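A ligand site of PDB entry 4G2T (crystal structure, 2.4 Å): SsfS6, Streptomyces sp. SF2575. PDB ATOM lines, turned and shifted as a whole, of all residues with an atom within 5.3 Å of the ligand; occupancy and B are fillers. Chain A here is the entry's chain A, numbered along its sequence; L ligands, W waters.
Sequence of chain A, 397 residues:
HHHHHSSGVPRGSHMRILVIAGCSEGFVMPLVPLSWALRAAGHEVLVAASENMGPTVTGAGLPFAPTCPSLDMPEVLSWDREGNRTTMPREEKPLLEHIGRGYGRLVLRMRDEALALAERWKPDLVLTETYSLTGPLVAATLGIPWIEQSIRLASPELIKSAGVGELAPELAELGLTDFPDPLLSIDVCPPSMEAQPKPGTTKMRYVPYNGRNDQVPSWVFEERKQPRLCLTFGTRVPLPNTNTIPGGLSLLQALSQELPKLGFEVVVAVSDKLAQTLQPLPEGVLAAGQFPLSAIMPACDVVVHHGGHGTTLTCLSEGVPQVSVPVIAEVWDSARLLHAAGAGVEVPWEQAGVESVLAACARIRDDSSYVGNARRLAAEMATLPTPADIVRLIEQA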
ATOM      1  N   SER A  24      25.060  13.496 -18.255  1.00  0.00           N
ATOM      2  CA  SER A  24      25.689  13.810 -19.541  1.00  0.00           C
ATOM      3  C   SER A  24      24.751  14.657 -20.400  1.00  0.00           C
ATOM      4  O   SER A  24      23.547  14.697 -20.149  1.00  0.00           O
ATOM      5  CB  SER A  24      26.118  12.537 -20.269  1.00  0.00           C
ATOM      6  OG  SER A  24      25.011  11.700 -20.557  1.00  0.00           O
ATOM      7  N   GLU A  25      25.318  15.328 -21.402  1.00  0.00           N
ATOM      8  CA  GLU A  25      24.588  16.309 -22.201  1.00  0.00           C
ATOM      9  C   GLU A  25      23.286  15.794 -22.806  1.00  0.00           C
ATOM     10  O   GLU A  25      22.319  16.530 -22.920  1.00  0.00           O
ATOM     11  CB  GLU A  25      25.493  16.856 -23.318  1.00  0.00           C
ATOM     12  CG  GLU A  25      26.693  17.647 -22.843  1.00  0.00           C
ATOM     13  CD  GLU A  25      27.893  16.769 -22.530  1.00  0.00           C
ATOM     14  OE1 GLU A  25      27.715  15.548 -22.341  1.00  0.00           O
ATOM     15  OE2 GLU A  25      29.021  17.302 -22.487  1.00  0.00           O
ATOM     16  N   GLY A  26      23.272  14.518 -23.177  1.00  0.00           N
ATOM     17  CA  GLY A  26      22.112  13.911 -23.810  1.00  0.00           C
ATOM     18  C   GLY A  26      20.896  13.809 -22.903  1.00  0.00           C
ATOM     19  O   GLY A  26      19.772  13.663 -23.377  1.00  0.00           O
ATOM     20  N   MET A  29      20.156  18.508 -22.180  1.00  0.00           N
ATOM     21  CA  MET A  29      19.722  19.359 -23.293  1.00  0.00           C
ATOM     22  C   MET A  29      18.247  19.242 -23.710  1.00  0.00           C
ATOM     23  O   MET A  29      17.602  20.259 -23.949  1.00  0.00           O
ATOM     24  CB  MET A  29      20.644  19.171 -24.497  1.00  0.00           C
ATOM     25  CG  MET A  29      22.087  19.591 -24.252  1.00  0.00           C
ATOM     26  SD  MET A  29      23.248  19.219 -25.770  1.00  0.00           S
ATOM     27  CE  MET A  29      24.896  20.013 -25.084  1.00  0.00           C
ATOM     28  N   TYR A 209      17.309  21.489 -28.740  1.00  0.00           N
ATOM     29  CA  TYR A 209      18.405  22.283 -28.212  1.00  0.00           C
ATOM     30  C   TYR A 209      19.663  21.427 -28.191  1.00  0.00           C
ATOM     31  O   TYR A 209      19.681  20.372 -27.551  1.00  0.00           O
ATOM     32  CB  TYR A 209      18.096  22.827 -26.816  1.00  0.00           C
ATOM     33  CG  TYR A 209      19.254  23.592 -26.227  1.00  0.00           C
ATOM     34  CD1 TYR A 209      19.567  24.867 -26.674  1.00  0.00           C
ATOM     35  CD2 TYR A 209      20.050  23.046 -25.231  1.00  0.00           C
ATOM     36  CE1 TYR A 209      20.634  25.574 -26.151  1.00  0.00           C
ATOM     37  CE2 TYR A 209      21.120  23.744 -24.697  1.00  0.00           C
ATOM     38  CZ  TYR A 209      21.403  25.015 -25.158  1.00  0.00           C
ATOM     39  OH  TYR A 209      22.464  25.717 -24.628  1.00  0.00           O
ATOM     40  N   ASN A 210      20.712  21.880 -28.866  1.00  0.00           N
ATOM     41  CA  ASN A 210      21.896  21.061 -29.068  1.00  0.00           C
ATOM     42  C   ASN A 210      23.177  21.643 -28.489  1.00  0.00           C
ATOM     43  O   ASN A 210      24.280  21.272 -28.896  1.00  0.00           O
ATOM     44  CB  ASN A 210      22.083  20.765 -30.557  1.00  0.00           C
ATOM     45  CG  ASN A 210      20.823  20.226 -31.208  1.00  0.00           C
ATOM     46  OD1 ASN A 210      20.300  20.830 -32.134  1.00  0.00           O
ATOM     47  ND2 ASN A 210      20.326  19.106 -30.702  1.00  0.00           N
ATOM     48  N   THR A 232      28.552  13.098 -36.965  1.00  0.00           N
ATOM     49  CA  THR A 232      28.616  13.320 -35.534  1.00  0.00           C
ATOM     50  C   THR A 232      28.341  12.039 -34.743  1.00  0.00           C
ATOM     51  O   THR A 232      27.485  11.241 -35.122  1.00  0.00           O
ATOM     52  CB  THR A 232      27.624  14.413 -35.077  1.00  0.00           C
ATOM     53  OG1 THR A 232      27.629  14.506 -33.647  1.00  0.00           O
ATOM     54  CG2 THR A 232      26.216  14.102 -35.563  1.00  0.00           C
ATOM     55  N   PHE A 233      29.070  11.839 -33.648  1.00  0.00           N
ATOM     56  CA  PHE A 233      28.870  10.661 -32.816  1.00  0.00           C
ATOM     57  C   PHE A 233      28.472  11.020 -31.384  1.00  0.00           C
ATOM     58  O   PHE A 233      28.456  10.158 -30.505  1.00  0.00           O
ATOM     59  CB  PHE A 233      30.125   9.768 -32.812  1.00  0.00           C
ATOM     60  CG  PHE A 233      30.241   8.894 -34.023  1.00  0.00           C
ATOM     61  CD1 PHE A 233      29.156   8.669 -34.857  1.00  0.00           C
ATOM     62  CD2 PHE A 233      31.440   8.271 -34.334  1.00  0.00           C
ATOM     63  CE1 PHE A 233      29.259   7.857 -35.966  1.00  0.00           C
ATOM     64  CE2 PHE A 233      31.557   7.460 -35.445  1.00  0.00           C
ATOM     65  CZ  PHE A 233      30.461   7.263 -36.266  1.00  0.00           C
ATOM     66  N   GLY A 234      28.127  12.277 -31.160  1.00  0.00           N
ATOM     67  CA  GLY A 234      27.635  12.721 -29.867  1.00  0.00           C
ATOM     68  C   GLY A 234      28.722  13.160 -28.902  1.00  0.00           C
ATOM     69  O   GLY A 234      29.790  13.620 -29.317  1.00  0.00           O
ATOM     70  N   THR A 235      28.455  13.011 -27.613  1.00  0.00           N
ATOM     71  CA  THR A 235      29.364  13.482 -26.575  1.00  0.00           C
ATOM     72  C   THR A 235      29.970  12.337 -25.770  1.00  0.00           C
ATOM     73  O   THR A 235      30.874  12.554 -24.962  1.00  0.00           O
ATOM     74  CB  THR A 235      28.647  14.434 -25.599  1.00  0.00           C
ATOM     75  OG1 THR A 235      27.649  13.707 -24.869  1.00  0.00           O
ATOM     76  CG2 THR A 235      27.976  15.575 -26.356  1.00  0.00           C
ATOM     77  N   ARG A 236      29.477  11.125 -26.010  1.00  0.00           N
ATOM     78  CA  ARG A 236      29.922   9.964 -25.251  1.00  0.00           C
ATOM     79  C   ARG A 236      30.705   8.983 -26.131  1.00  0.00           C
ATOM     80  O   ARG A 236      31.797   8.549 -25.754  1.00  0.00           O
ATOM     81  CB  ARG A 236      28.722   9.258 -24.621  1.00  0.00           C
ATOM     82  CG  ARG A 236      27.860  10.178 -23.768  1.00  0.00           C
ATOM     83  CD  ARG A 236      26.429   9.671 -23.696  1.00  0.00           C
ATOM     84  NE  ARG A 236      26.311   8.421 -22.945  1.00  0.00           N
ATOM     85  CZ  ARG A 236      25.189   7.715 -22.858  1.00  0.00           C
ATOM     86  NH1 ARG A 236      24.089   8.130 -23.461  1.00  0.00           N
ATOM     87  NH2 ARG A 236      25.173   6.591 -22.162  1.00  0.00           N
ATOM     88  N   VAL A 237      30.137   8.644 -27.275  1.00  0.00           N
ATOM     89  CA  VAL A 237      30.785   7.735 -28.231  1.00  0.00           C
ATOM     90  C   VAL A 237      32.190   8.202 -28.655  1.00  0.00           C
ATOM     91  O   VAL A 237      33.110   7.382 -28.700  1.00  0.00           O
ATOM     92  CB  VAL A 237      29.883   7.444 -29.459  1.00  0.00           C
ATOM     93  CG1 VAL A 237      30.660   6.717 -30.544  1.00  0.00           C
ATOM     94  CG2 VAL A 237      28.661   6.641 -29.037  1.00  0.00           C
ATOM     95  N   ALA A 269      30.587  17.279 -36.543  1.00  0.00           N
ATOM     96  CA  ALA A 269      30.169  17.830 -35.269  1.00  0.00           C
ATOM     97  C   ALA A 269      30.698  16.988 -34.125  1.00  0.00           C
ATOM     98  O   ALA A 269      30.154  15.925 -33.817  1.00  0.00           O
ATOM     99  CB  ALA A 269      28.652  17.939 -35.208  1.00  0.00           C
ATOM    100  N   VAL A 270      31.772  17.453 -33.496  1.00  0.00           N
ATOM    101  CA  VAL A 270      32.441  16.707 -32.448  1.00  0.00           C
ATOM    102  C   VAL A 270      33.104  17.709 -31.491  1.00  0.00           C
ATOM    103  O   VAL A 270      33.258  18.873 -31.841  1.00  0.00           O
ATOM    104  CB  VAL A 270      33.492  15.739 -33.032  1.00  0.00           C
ATOM    105  CG1 VAL A 270      34.700  16.514 -33.552  1.00  0.00           C
ATOM    106  CG2 VAL A 270      33.911  14.678 -32.025  1.00  0.00           C
ATOM    107  N   SER A 271      33.474  17.254 -30.296  1.00  0.00           N
ATOM    108  CA  SER A 271      34.120  18.112 -29.316  1.00  0.00           C
ATOM    109  C   SER A 271      35.340  18.820 -29.897  1.00  0.00           C
ATOM    110  O   SER A 271      36.093  18.224 -30.675  1.00  0.00           O
ATOM    111  CB  SER A 271      34.523  17.314 -28.077  1.00  0.00           C
ATOM    112  OG  SER A 271      35.166  18.126 -27.121  1.00  0.00           O
ATOM    113  N   GLY A 289      34.283  20.534 -35.547  1.00  0.00           N
ATOM    114  CA  GLY A 289      34.216  21.165 -34.241  1.00  0.00           C
ATOM    115  C   GLY A 289      32.826  21.112 -33.650  1.00  0.00           C
ATOM    116  O   GLY A 289      31.927  20.469 -34.192  1.00  0.00           O
ATOM    117  N   GLN A 290      32.655  21.785 -32.512  1.00  0.00           N
ATOM    118  CA  GLN A 290      31.372  21.808 -31.828  1.00  0.00           C
ATOM    119  C   GLN A 290      30.347  22.661 -32.555  1.00  0.00           C
ATOM    120  O   GLN A 290      30.441  23.888 -32.578  1.00  0.00           O
ATOM    121  CB  GLN A 290      31.540  22.323 -30.393  1.00  0.00           C
ATOM    122  CG  GLN A 290      31.566  21.231 -29.336  1.00  0.00           C
ATOM    123  CD  GLN A 290      30.190  20.712 -28.991  1.00  0.00           C
ATOM    124  OE1 GLN A 290      29.172  21.275 -29.416  1.00  0.00           O
ATOM    125  NE2 GLN A 290      30.126  19.639 -28.203  1.00  0.00           N
ATOM    126  N   PHE A 291      29.365  21.995 -33.157  1.00  0.00           N
ATOM    127  CA  PHE A 291      28.271  22.694 -33.821  1.00  0.00           C
ATOM    128  C   PHE A 291      26.929  22.135 -33.353  1.00  0.00           C
ATOM    129  O   PHE A 291      26.613  20.969 -33.618  1.00  0.00           O
ATOM    130  CB  PHE A 291      28.369  22.567 -35.345  1.00  0.00           C
ATOM    131  CG  PHE A 291      29.703  22.983 -35.907  1.00  0.00           C
ATOM    132  CD1 PHE A 291      30.088  24.313 -35.885  1.00  0.00           C
ATOM    133  CD2 PHE A 291      30.549  22.047 -36.473  1.00  0.00           C
ATOM    134  CE1 PHE A 291      31.301  24.699 -36.405  1.00  0.00           C
ATOM    135  CE2 PHE A 291      31.770  22.431 -36.988  1.00  0.00           C
ATOM    136  CZ  PHE A 291      32.150  23.756 -36.960  1.00  0.00           C
ATOM    137  N   PRO A 292      26.145  22.960 -32.650  1.00  0.00           N
ATOM    138  CA  PRO A 292      24.764  22.602 -32.302  1.00  0.00           C
ATOM    139  C   PRO A 292      24.011  22.246 -33.577  1.00  0.00           C
ATOM    140  O   PRO A 292      23.921  23.079 -34.479  1.00  0.00           O
ATOM    141  CB  PRO A 292      24.218  23.894 -31.694  1.00  0.00           C
ATOM    142  CG  PRO A 292      25.417  24.567 -31.128  1.00  0.00           C
ATOM    143  CD  PRO A 292      26.537  24.258 -32.083  1.00  0.00           C
ATOM    144  N   LEU A 293      23.505  21.022 -33.635  1.00  0.00           N
ATOM    145  CA  LEU A 293      22.930  20.486 -34.868  1.00  0.00           C
ATOM    146  C   LEU A 293      21.822  21.358 -35.464  1.00  0.00           C
ATOM    147  O   LEU A 293      21.799  21.575 -36.673  1.00  0.00           O
ATOM    148  CB  LEU A 293      22.423  19.058 -34.639  1.00  0.00           C
ATOM    149  CG  LEU A 293      23.510  18.051 -34.235  1.00  0.00           C
ATOM    150  CD1 LEU A 293      22.931  16.646 -34.160  1.00  0.00           C
ATOM    151  CD2 LEU A 293      24.687  18.099 -35.191  1.00  0.00           C
ATOM    152  N   HIS A 306      25.575   8.113 -34.429  1.00  0.00           N
ATOM    153  CA  HIS A 306      25.709   6.944 -33.559  1.00  0.00           C
ATOM    154  C   HIS A 306      24.367   6.478 -33.014  1.00  0.00           C
ATOM    155  O   HIS A 306      24.312   5.679 -32.072  1.00  0.00           O
ATOM    156  CB  HIS A 306      26.634   7.277 -32.386  1.00  0.00           C
ATOM    157  CG  HIS A 306      26.072   8.305 -31.460  1.00  0.00           C
ATOM    158  ND1 HIS A 306      25.741   9.584 -31.865  1.00  0.00           N
ATOM    159  CD2 HIS A 306      25.786   8.255 -30.139  1.00  0.00           C
ATOM    160  CE1 HIS A 306      25.266  10.270 -30.843  1.00  0.00           C
ATOM    161  NE2 HIS A 306      25.288   9.483 -29.776  1.00  0.00           N
ATOM    162  N   GLY A 308      22.278   8.353 -31.493  1.00  0.00           N
ATOM    163  CA  GLY A 308      21.982   9.120 -30.294  1.00  0.00           C
ATOM    164  C   GLY A 308      20.577   9.691 -30.303  1.00  0.00           C
ATOM    165  O   GLY A 308      20.123  10.206 -31.319  1.00  0.00           O
ATOM    166  N   HIS A 309      19.899   9.589 -29.153  1.00  0.00           N
ATOM    167  CA  HIS A 309      18.502  10.017 -29.037  1.00  0.00           C
ATOM    168  C   HIS A 309      18.300  11.474 -29.448  1.00  0.00           C
ATOM    169  O   HIS A 309      17.420  11.770 -30.269  1.00  0.00           O
ATOM    170  CB  HIS A 309      18.009   9.807 -27.608  1.00  0.00           C
ATOM    171  CG  HIS A 309      17.716   8.377 -27.269  1.00  0.00           C
ATOM    172  ND1 HIS A 309      18.121   7.787 -26.091  1.00  0.00           N
ATOM    173  CD2 HIS A 309      17.060   7.418 -27.964  1.00  0.00           C
ATOM    174  CE1 HIS A 309      17.728   6.530 -26.076  1.00  0.00           C
ATOM    175  NE2 HIS A 309      17.078   6.275 -27.192  1.00  0.00           N
ATOM    176  N   GLY A 310      19.101  12.374 -28.892  1.00  0.00           N
ATOM    177  CA  GLY A 310      19.005  13.779 -29.204  1.00  0.00           C
ATOM    178  C   GLY A 310      19.368  14.076 -30.647  1.00  0.00           C
ATOM    179  O   GLY A 310      18.729  14.897 -31.308  1.00  0.00           O
ATOM    180  N   THR A 311      20.410  13.401 -31.139  1.00  0.00           N
ATOM    181  CA  THR A 311      20.858  13.577 -32.512  1.00  0.00           C
ATOM    182  C   THR A 311      19.793  13.113 -33.508  1.00  0.00           C
ATOM    183  O   THR A 311      19.541  13.762 -34.517  1.00  0.00           O
ATOM    184  CB  THR A 311      22.170  12.814 -32.774  1.00  0.00           C
ATOM    185  OG1 THR A 311      23.184  13.302 -31.881  1.00  0.00           O
ATOM    186  CG2 THR A 311      22.632  12.998 -34.206  1.00  0.00           C
ATOM    187  N   THR A 312      19.161  11.977 -33.198  1.00  0.00           N
ATOM    188  CA  THR A 312      18.133  11.420 -34.066  1.00  0.00           C
ATOM    189  C   THR A 312      16.906  12.315 -34.137  1.00  0.00           C
ATOM    190  O   THR A 312      16.419  12.628 -35.223  1.00  0.00           O
ATOM    191  CB  THR A 312      17.701  10.017 -33.578  1.00  0.00           C
ATOM    192  OG1 THR A 312      18.833   9.149 -33.537  1.00  0.00           O
ATOM    193  CG2 THR A 312      16.655   9.426 -34.521  1.00  0.00           C
ATOM    194  N   THR A 314      16.653  15.482 -33.409  1.00  0.00           N
ATOM    195  CA  THR A 314      16.992  16.774 -33.992  1.00  0.00           C
ATOM    196  C   THR A 314      17.032  16.700 -35.508  1.00  0.00           C
ATOM    197  O   THR A 314      16.471  17.559 -36.195  1.00  0.00           O
ATOM    198  CB  THR A 314      18.341  17.306 -33.456  1.00  0.00           C
ATOM    199  OG1 THR A 314      18.253  17.516 -32.043  1.00  0.00           O
ATOM    200  CG2 THR A 314      18.709  18.614 -34.142  1.00  0.00           C
ATOM    201  N   ILE A 328      24.797   2.421 -28.464  1.00  0.00           N
ATOM    202  CA  ILE A 328      24.249   2.114 -27.146  1.00  0.00           C
ATOM    203  C   ILE A 328      22.942   1.344 -27.260  1.00  0.00           C
ATOM    204  O   ILE A 328      22.140   1.592 -28.161  1.00  0.00           O
ATOM    205  CB  ILE A 328      24.070   3.387 -26.307  1.00  0.00           C
ATOM    206  CG1 ILE A 328      25.399   4.141 -26.219  1.00  0.00           C
ATOM    207  CG2 ILE A 328      23.552   3.079 -24.917  1.00  0.00           C
ATOM    208  CD1 ILE A 328      25.348   5.388 -25.365  1.00  0.00           C
HETATM  209  P1  LIG L   1      22.751  12.381 -28.063  1.00  0.00           P
HETATM  210  O1  LIG L   1      22.246  12.585 -29.474  1.00  0.00           O
HETATM  211  O2  LIG L   1      21.680  11.738 -27.220  1.00  0.00           O
HETATM  212  O3  LIG L   1      24.028  11.485 -28.120  1.00  0.00           O
HETATM  213  P2  LIG L   1      24.830  11.158 -26.814  1.00  0.00           P
HETATM  214  O4  LIG L   1      23.881  11.098 -25.633  1.00  0.00           O
HETATM  215  O5  LIG L   1      25.496   9.817 -26.994  1.00  0.00           O
HETATM  216  O6  LIG L   1      25.865  12.224 -26.572  1.00  0.00           O
HETATM  217  O7  LIG L   1      23.151  13.752 -27.444  1.00  0.00           O
HETATM  218  C1  LIG L   1      24.033  14.579 -28.101  1.00  0.00           C
HETATM  219  C2  LIG L   1      23.541  15.987 -28.009  1.00  0.00           C
HETATM  220  O8  LIG L   1      24.603  16.866 -28.133  1.00  0.00           O
HETATM  221  C3  LIG L   1      22.600  16.266 -29.149  1.00  0.00           C
HETATM  222  O9  LIG L   1      21.630  17.154 -28.732  1.00  0.00           O
HETATM  223  C4  LIG L   1      23.422  16.845 -30.250  1.00  0.00           C
HETATM  224  C5  LIG L   1      24.533  17.582 -29.411  1.00  0.00           C
HETATM  225  N1  LIG L   1      25.854  17.922 -30.141  1.00  0.00           N
HETATM  226  C6  LIG L   1      25.931  18.914 -31.188  1.00  0.00           C
HETATM  227  O10 LIG L   1      24.931  19.511 -31.538  1.00  0.00           O
HETATM  228  N2  LIG L   1      27.151  19.211 -31.838  1.00  0.00           N
HETATM  229  C7  LIG L   1      28.318  18.537 -31.467  1.00  0.00           C
HETATM  230  O11 LIG L   1      29.388  18.795 -32.030  1.00  0.00           O
HETATM  231  C8  LIG L   1      28.256  17.517 -30.381  1.00  0.00           C
HETATM  232  C9  LIG L   1      29.503  16.813 -29.979  1.00  0.00           C
HETATM  233  C10 LIG L   1      27.069  17.230 -29.741  1.00  0.00           C
HETATM  234  O   HOH W   1      25.481  12.844 -23.517  1.00  0.00           O
HETATM  235  O   HOH W   2      21.318   9.069 -26.641  1.00  0.00           O
HETATM  236  O   HOH W   3      19.296  13.618 -25.939  1.00  0.00           O
HETATM  237  O   HOH W   4      27.859   9.719 -27.864  1.00  0.00           O
HETATM  238  O   HOH W   5      20.205  16.370 -26.921  1.00  0.00           O
HETATM  239  O   HOH W   6      32.098  14.896 -29.186  1.00  0.00           O
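The backbone NH (N) of Phe 291 lies within hydrogen-bond range of an oxygen (O11) of the ligand (3.4 Å).
The backbone carbonyl oxygen (O) of Phe 291 sits at hydrogen-bond distance from a nitrogen (N2) of the ligand, at 2.6 Å.
The backbone NH of Thr 311 is in hydrogen-bond range of an oxygen (O1) of the ligand (2.6 Å).
The side-chain hydroxyl (OG1) of Thr 311 lies within hydrogen-bond range of an oxygen (O1) of the ligand (2.7 Å).
A ring nitrogen (NE2) of His 306 lies within hydrogen-bond range of an oxygen (O5) of the ligand.
N of Thr 235 lies within hydrogen-bond range of O6 of the ligand.
OG1 of Thr 235 is in hydrogen-bond range of O6 of the ligand.
N of Leu 293 lies within hydrogen-bond range of O10 of the ligand (3.0 Å).
An oxygen (O9) of the ligand lies within hydrogen-bond range of the side-chain amide nitrogen (ND2) of Asn 210 (3.1 Å).
The backbone NH (N) of Val 270 lies within hydrogen-bond range of an oxygen (O11) of the ligand (3.1 Å).
N of Gly 310 lies within hydrogen-bond range of O2 of the ligand (3.1 Å).
The backbone NH of His 309 sits at hydrogen-bond distance from an oxygen (O2) of the ligand (3.4 Å).
An oxygen (O4) of the ligand lies within salt-bridge range of the guanidinium group of Arg 236, at 3.7 Å.
SD of Met 29 lies close to O8 of the ligand (3.6 Å).
O of Ala 269 lies close to O11 of the ligand, 3.5 Å away.
Merely in contact with the ligand: Pro 292, Gly 234, Gln 290, Gly 308, Gly 289, Gly 26 and Tyr 209.
Hydrophobic or aromatic side chains within 4 Å of the ligand: Met 29, Ala 269, Leu 293 and His 306.
Within 4 Å of the ligand: Gly 26, Met 29, Tyr 209, Asn 210, Gly 234, Thr 235, Arg 236, Ala 269, Val 270, Gly 289, Gln 290, Phe 291, Pro 292, Leu 293, His 306, Gly 308, His 309, Gly 310 and Thr 311.
The nearest printed residue that does not touch the ligand is Ser 271 (4.01 Å).
O of Phe 233 lies within hydrogen-bond range of ND1 of His 306, at 3.1 Å.
The side-chain hydroxyl (OG1) of Thr 235 is in hydrogen-bond range of the side-chain carboxylate (OE1) of Glu 25 (3.1 Å).
OG1 of Thr 232 sits at hydrogen-bond distance from O of Ala 269 (2.9 Å).
N of Gln 290 is in hydrogen-bond range of O of Val 270, 3.0 Å away.
The backbone NH (N) of Val 270 is in hydrogen-bond range of the backbone carbonyl oxygen (O) of Gly 289, at 3.1 Å.
The backbone carbonyl oxygen (O) of Gly 310 sits at hydrogen-bond distance from the side-chain hydroxyl (OG1) of Thr 314.
The backbone NH (N) of Gly 234 lies within hydrogen-bond range of the side-chain hydroxyl (OG1) of Thr 232 (3.4 Å).
The backbone carbonyl oxygen of Gly 308 sits at hydrogen-bond distance from the side-chain hydroxyl of Thr 312.
Water W2 bridges an oxygen (O2) of the ligand (2.8 Å) and the backbone NH (N) of His 309 (2.9 Å).
Water W1 lies within hydrogen-bond range of the side-chain hydroxyl (OG1) of Thr 235, the backbone NH (N) of Gly 26, an oxygen (O6) of the ligand, the side-chain hydroxyl (OG) of Ser 24 and the backbone NH (N) of Glu 25.
Water W3 lies within hydrogen-bond range of O of Gly 26 (2.6 Å), N of Gly 310 (3.2 Å) and O2 of the ligand (3.3 Å).
Water W6 bridges O of Gly 234 (2.6 Å) and N of Ser 271 (2.9 Å).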
